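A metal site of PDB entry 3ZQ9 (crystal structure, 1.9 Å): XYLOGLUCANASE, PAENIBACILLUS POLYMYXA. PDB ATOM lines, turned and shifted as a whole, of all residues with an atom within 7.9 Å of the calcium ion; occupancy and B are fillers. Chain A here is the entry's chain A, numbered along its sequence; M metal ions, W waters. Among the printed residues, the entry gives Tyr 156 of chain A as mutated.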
ATOM      1  N   ASN A  54       5.397  14.721 -21.405  1.00  0.00           N
ATOM      2  CA  ASN A  54       4.337  15.588 -20.939  1.00  0.00           C
ATOM      3  C   ASN A  54       4.812  17.010 -21.193  1.00  0.00           C
ATOM      4  O   ASN A  54       5.741  17.465 -20.548  1.00  0.00           O
ATOM      5  CB  ASN A  54       4.184  15.375 -19.429  1.00  0.00           C
ATOM      6  CG  ASN A  54       3.142  16.297 -18.786  1.00  0.00           C
ATOM      7  OD1 ASN A  54       2.822  17.340 -19.339  1.00  0.00           O
ATOM      8  ND2 ASN A  54       2.638  15.911 -17.598  1.00  0.00           N
ATOM      9  N   TRP A  55       4.188  17.700 -22.141  1.00  0.00           N
ATOM     10  CA  TRP A  55       4.716  19.043 -22.513  1.00  0.00           C
ATOM     11  C   TRP A  55       4.568  20.055 -21.371  1.00  0.00           C
ATOM     12  O   TRP A  55       5.289  21.068 -21.341  1.00  0.00           O
ATOM     13  CB  TRP A  55       4.006  19.539 -23.775  1.00  0.00           C
ATOM     14  CG  TRP A  55       2.620  20.112 -23.537  1.00  0.00           C
ATOM     15  CD1 TRP A  55       1.429  19.426 -23.484  1.00  0.00           C
ATOM     16  CD2 TRP A  55       2.282  21.517 -23.409  1.00  0.00           C
ATOM     17  NE1 TRP A  55       0.383  20.333 -23.274  1.00  0.00           N
ATOM     18  CE2 TRP A  55       0.884  21.605 -23.224  1.00  0.00           C
ATOM     19  CE3 TRP A  55       3.046  22.686 -23.385  1.00  0.00           C
ATOM     20  CZ2 TRP A  55       0.222  22.854 -23.073  1.00  0.00           C
ATOM     21  CZ3 TRP A  55       2.384  23.926 -23.229  1.00  0.00           C
ATOM     22  CH2 TRP A  55       0.994  23.987 -23.075  1.00  0.00           C
ATOM     23  N   GLU A  56       3.632  19.800 -20.449  1.00  0.00           N
ATOM     24  CA  GLU A  56       3.377  20.791 -19.387  1.00  0.00           C
ATOM     25  C   GLU A  56       4.528  20.907 -18.407  1.00  0.00           C
ATOM     26  O   GLU A  56       4.782  22.010 -17.875  1.00  0.00           O
ATOM     27  CB  GLU A  56       2.081  20.458 -18.619  1.00  0.00           C
ATOM     28  CG  GLU A  56       0.857  20.388 -19.524  1.00  0.00           C
ATOM     29  CD  GLU A  56      -0.411  20.108 -18.719  1.00  0.00           C
ATOM     30  OE1 GLU A  56      -0.289  19.627 -17.562  1.00  0.00           O
ATOM     31  OE2 GLU A  56      -1.524  20.345 -19.241  1.00  0.00           O
ATOM     32  N   LYS A 118       3.179  11.936 -15.316  1.00  0.00           N
ATOM     33  CA  LYS A 118       2.726  13.016 -14.420  1.00  0.00           C
ATOM     34  C   LYS A 118       3.871  13.665 -13.626  1.00  0.00           C
ATOM     35  O   LYS A 118       3.800  14.845 -13.208  1.00  0.00           O
ATOM     36  CB  LYS A 118       1.633  12.491 -13.470  1.00  0.00           C
ATOM     37  CG  LYS A 118       0.824  13.581 -12.707  1.00  0.00           C
ATOM     38  CD  LYS A 118      -0.502  12.928 -12.153  1.00  0.00           C
ATOM     39  CE  LYS A 118      -1.294  13.937 -11.330  1.00  0.00           C
ATOM     40  NZ  LYS A 118      -1.839  15.102 -12.139  1.00  0.00           N
ATOM     41  N   ASN A 136      -0.812  11.220 -16.424  1.00  0.00           N
ATOM     42  CA  ASN A 136      -1.944  12.050 -16.853  1.00  0.00           C
ATOM     43  C   ASN A 136      -2.510  11.451 -18.148  1.00  0.00           C
ATOM     44  O   ASN A 136      -1.774  10.843 -18.924  1.00  0.00           O
ATOM     45  CB  ASN A 136      -1.463  13.481 -17.157  1.00  0.00           C
ATOM     46  CG  ASN A 136      -1.173  14.271 -15.909  1.00  0.00           C
ATOM     47  OD1 ASN A 136      -1.823  14.095 -14.894  1.00  0.00           O
ATOM     48  ND2 ASN A 136      -0.210  15.173 -15.985  1.00  0.00           N
ATOM     49  N   GLN A 137      -3.784  11.647 -18.403  1.00  0.00           N
ATOM     50  CA  GLN A 137      -4.358  11.148 -19.653  1.00  0.00           C
ATOM     51  C   GLN A 137      -4.263  12.167 -20.754  1.00  0.00           C
ATOM     52  O   GLN A 137      -4.387  13.376 -20.498  1.00  0.00           O
ATOM     53  CB  GLN A 137      -5.803  10.659 -19.456  1.00  0.00           C
ATOM     54  CG  GLN A 137      -6.759  11.626 -18.975  1.00  0.00           C
ATOM     55  CD  GLN A 137      -8.019  10.871 -18.448  1.00  0.00           C
ATOM     56  OE1 GLN A 137      -8.238  10.777 -17.234  1.00  0.00           O
ATOM     57  NE2 GLN A 137      -8.780  10.289 -19.338  1.00  0.00           N
ATOM     58  N   LYS A 142      -8.964  20.061 -26.584  1.00  0.00           N
ATOM     59  CA  LYS A 142      -9.381  20.549 -25.287  1.00  0.00           C
ATOM     60  C   LYS A 142     -10.853  20.991 -25.260  1.00  0.00           C
ATOM     61  O   LYS A 142     -11.547  20.842 -24.232  1.00  0.00           O
ATOM     62  CB  LYS A 142      -8.490  21.729 -24.889  1.00  0.00           C
ATOM     63  CG  LYS A 142      -8.715  22.195 -23.424  1.00  0.00           C
ATOM     64  CD  LYS A 142      -7.829  23.409 -23.117  1.00  0.00           C
ATOM     65  CE  LYS A 142      -7.873  23.665 -21.571  1.00  0.00           C
ATOM     66  NZ  LYS A 142      -7.137  24.930 -21.218  1.00  0.00           N
ATOM     67  N   GLN A 147      -4.767  27.693 -22.683  1.00  0.00           N
ATOM     68  CA  GLN A 147      -3.908  28.417 -21.764  1.00  0.00           C
ATOM     69  C   GLN A 147      -2.467  28.278 -22.256  1.00  0.00           C
ATOM     70  O   GLN A 147      -2.004  27.170 -22.514  1.00  0.00           O
ATOM     71  CB  GLN A 147      -4.030  27.810 -20.327  1.00  0.00           C
ATOM     72  CG  GLN A 147      -5.488  27.833 -19.776  1.00  0.00           C
ATOM     73  CD  GLN A 147      -5.706  26.944 -18.519  1.00  0.00           C
ATOM     74  OE1 GLN A 147      -5.689  27.442 -17.387  1.00  0.00           O
ATOM     75  NE2 GLN A 147      -5.951  25.634 -18.727  1.00  0.00           N
ATOM     76  N   PRO A 150      -0.464  26.058 -18.984  1.00  0.00           N
ATOM     77  CA  PRO A 150      -1.490  25.012 -18.833  1.00  0.00           C
ATOM     78  C   PRO A 150      -1.716  24.672 -17.370  1.00  0.00           C
ATOM     79  O   PRO A 150      -0.846  24.911 -16.504  1.00  0.00           O
ATOM     80  CB  PRO A 150      -0.862  23.805 -19.569  1.00  0.00           C
ATOM     81  CG  PRO A 150       0.670  24.046 -19.420  1.00  0.00           C
ATOM     82  CD  PRO A 150       0.736  25.557 -19.690  1.00  0.00           C
ATOM     83  N   ASP A 151      -2.878  24.100 -17.090  1.00  0.00           N
ATOM     84  CA  ASP A 151      -3.231  23.706 -15.749  1.00  0.00           C
ATOM     85  C   ASP A 151      -2.365  22.506 -15.324  1.00  0.00           C
ATOM     86  O   ASP A 151      -2.438  21.427 -15.911  1.00  0.00           O
ATOM     87  CB  ASP A 151      -4.715  23.311 -15.763  1.00  0.00           C
ATOM     88  CG  ASP A 151      -5.269  23.025 -14.393  1.00  0.00           C
ATOM     89  OD1 ASP A 151      -4.533  22.615 -13.475  1.00  0.00           O
ATOM     90  OD2 ASP A 151      -6.513  23.187 -14.251  1.00  0.00           O
ATOM     91  N   LEU A 152      -1.553  22.716 -14.290  1.00  0.00           N
ATOM     92  CA  LEU A 152      -0.585  21.689 -13.861  1.00  0.00           C
ATOM     93  C   LEU A 152      -1.164  20.714 -12.839  1.00  0.00           C
ATOM     94  O   LEU A 152      -0.523  19.696 -12.504  1.00  0.00           O
ATOM     95  CB  LEU A 152       0.678  22.352 -13.295  1.00  0.00           C
ATOM     96  CG  LEU A 152       1.427  23.298 -14.229  1.00  0.00           C
ATOM     97  CD1 LEU A 152       2.663  23.877 -13.516  1.00  0.00           C
ATOM     98  CD2 LEU A 152       1.883  22.590 -15.523  1.00  0.00           C
ATOM     99  N   ASN A 153      -2.368  21.019 -12.345  1.00  0.00           N
ATOM    100  CA  ASN A 153      -2.944  20.258 -11.231  1.00  0.00           C
ATOM    101  C   ASN A 153      -4.064  19.298 -11.595  1.00  0.00           C
ATOM    102  O   ASN A 153      -4.528  18.535 -10.740  1.00  0.00           O
ATOM    103  CB  ASN A 153      -3.381  21.224 -10.138  1.00  0.00           C
ATOM    104  CG  ASN A 153      -2.189  21.964  -9.548  1.00  0.00           C
ATOM    105  OD1 ASN A 153      -2.216  23.167  -9.399  1.00  0.00           O
ATOM    106  ND2 ASN A 153      -1.125  21.228  -9.284  1.00  0.00           N
ATOM    107  N   ASP A 154      -4.456  19.278 -12.863  1.00  0.00           N
ATOM    108  CA  ASP A 154      -5.485  18.350 -13.282  1.00  0.00           C
ATOM    109  C   ASP A 154      -4.840  17.067 -13.790  1.00  0.00           C
ATOM    110  O   ASP A 154      -3.604  16.902 -13.740  1.00  0.00           O
ATOM    111  CB  ASP A 154      -6.436  19.003 -14.326  1.00  0.00           C
ATOM    112  CG  ASP A 154      -5.727  19.370 -15.634  1.00  0.00           C
ATOM    113  OD1 ASP A 154      -4.548  18.982 -15.845  1.00  0.00           O
ATOM    114  OD2 ASP A 154      -6.382  20.029 -16.485  1.00  0.00           O
ATOM    115  N   ASN A 155      -5.669  16.162 -14.314  1.00  0.00           N
ATOM    116  CA  ASN A 155      -5.189  14.847 -14.719  1.00  0.00           C
ATOM    117  C   ASN A 155      -4.970  14.753 -16.244  1.00  0.00           C
ATOM    118  O   ASN A 155      -4.957  13.662 -16.795  1.00  0.00           O
ATOM    119  CB  ASN A 155      -6.224  13.803 -14.318  1.00  0.00           C
ATOM    120  CG  ASN A 155      -5.612  12.448 -14.163  1.00  0.00           C
ATOM    121  OD1 ASN A 155      -4.583  12.325 -13.519  1.00  0.00           O
ATOM    122  ND2 ASN A 155      -6.175  11.451 -14.865  1.00  0.00           N
ATOM    123  N   TYR A 156      -4.846  15.912 -16.911  1.00  0.00           N
ATOM    124  CA  TYR A 156      -4.890  15.913 -18.382  1.00  0.00           C
ATOM    125  C   TYR A 156      -3.736  16.638 -18.983  1.00  0.00           C
ATOM    126  O   TYR A 156      -3.246  17.600 -18.412  1.00  0.00           O
ATOM    127  CB  TYR A 156      -6.144  16.684 -18.855  1.00  0.00           C
ATOM    128  CG  TYR A 156      -7.415  16.036 -18.361  1.00  0.00           C
ATOM    129  CD1 TYR A 156      -7.853  14.824 -18.920  1.00  0.00           C
ATOM    130  CD2 TYR A 156      -8.116  16.561 -17.260  1.00  0.00           C
ATOM    131  CE1 TYR A 156      -9.026  14.161 -18.418  1.00  0.00           C
ATOM    132  CE2 TYR A 156      -9.271  15.902 -16.751  1.00  0.00           C
ATOM    133  CZ  TYR A 156      -9.711  14.744 -17.337  1.00  0.00           C
ATOM    134  OH  TYR A 156     -10.823  14.102 -16.888  1.00  0.00           O
ATOM    135  N   VAL A 157      -3.360  16.227 -20.191  1.00  0.00           N
ATOM    136  CA  VAL A 157      -2.594  17.073 -21.082  1.00  0.00           C
ATOM    137  C   VAL A 157      -3.410  17.160 -22.394  1.00  0.00           C
ATOM    138  O   VAL A 157      -3.955  16.154 -22.826  1.00  0.00           O
ATOM    139  CB  VAL A 157      -1.210  16.478 -21.273  1.00  0.00           C
ATOM    140  CG1 VAL A 157      -0.470  17.166 -22.343  1.00  0.00           C
ATOM    141  CG2 VAL A 157      -0.421  16.532 -19.945  1.00  0.00           C
ATOM    142  N   TYR A 158      -3.518  18.359 -22.965  1.00  0.00           N
ATOM    143  CA  TYR A 158      -4.316  18.550 -24.160  1.00  0.00           C
ATOM    144  C   TYR A 158      -3.380  18.773 -25.347  1.00  0.00           C
ATOM    145  O   TYR A 158      -2.603  19.725 -25.309  1.00  0.00           O
ATOM    146  CB  TYR A 158      -5.196  19.776 -23.972  1.00  0.00           C
ATOM    147  CG  TYR A 158      -6.249  19.574 -22.891  1.00  0.00           C
ATOM    148  CD1 TYR A 158      -7.353  18.761 -23.098  1.00  0.00           C
ATOM    149  CD2 TYR A 158      -6.097  20.210 -21.650  1.00  0.00           C
ATOM    150  CE1 TYR A 158      -8.338  18.590 -22.071  1.00  0.00           C
ATOM    151  CE2 TYR A 158      -7.059  20.022 -20.615  1.00  0.00           C
ATOM    152  CZ  TYR A 158      -8.165  19.226 -20.856  1.00  0.00           C
ATOM    153  OH  TYR A 158      -9.105  19.093 -19.824  1.00  0.00           O
ATOM    154  N   GLU A 161      -3.783  22.091 -27.341  1.00  0.00           N
ATOM    155  CA  GLU A 161      -3.259  23.211 -26.524  1.00  0.00           C
ATOM    156  C   GLU A 161      -1.741  23.355 -26.677  1.00  0.00           C
ATOM    157  O   GLU A 161      -1.208  24.477 -26.708  1.00  0.00           O
ATOM    158  CB  GLU A 161      -3.607  22.959 -25.055  1.00  0.00           C
ATOM    159  CG  GLU A 161      -3.237  24.144 -24.164  1.00  0.00           C
ATOM    160  CD  GLU A 161      -3.946  24.044 -22.815  1.00  0.00           C
ATOM    161  OE1 GLU A 161      -3.683  23.091 -22.054  1.00  0.00           O
ATOM    162  OE2 GLU A 161      -4.742  24.975 -22.528  1.00  0.00           O
HETATM  163 CA    CA M   1      -2.739  19.543 -17.246  1.00  0.00          CA
HETATM  164  O   HOH W   1      -4.565  20.666 -18.405  1.00  0.00           O
HETATM  165  O   HOH W   2      -1.895  18.233 -15.427  1.00  0.00           O
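N of Asn 153 is in hydrogen-bond range of OD1 of Asp 151 (2.9 Å). The side-chain amino group of Lys 118 sits at hydrogen-bond distance from the backbone carbonyl oxygen of Asp 154, at 3.0 Å. The backbone NH (N) of Glu 56 lies within hydrogen-bond range of the side-chain amide oxygen (OD1) of Asn 54, at 2.8 Å.
Of the 18 residues printed, 4 come within 4 Å of the calcium ion.
The calcium ion is bound by O of Tyr 156, O of Asp 151, OD1 of Asp 154, water W2, water W1, OE2 of Glu 56 and OE1 of Glu 56.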
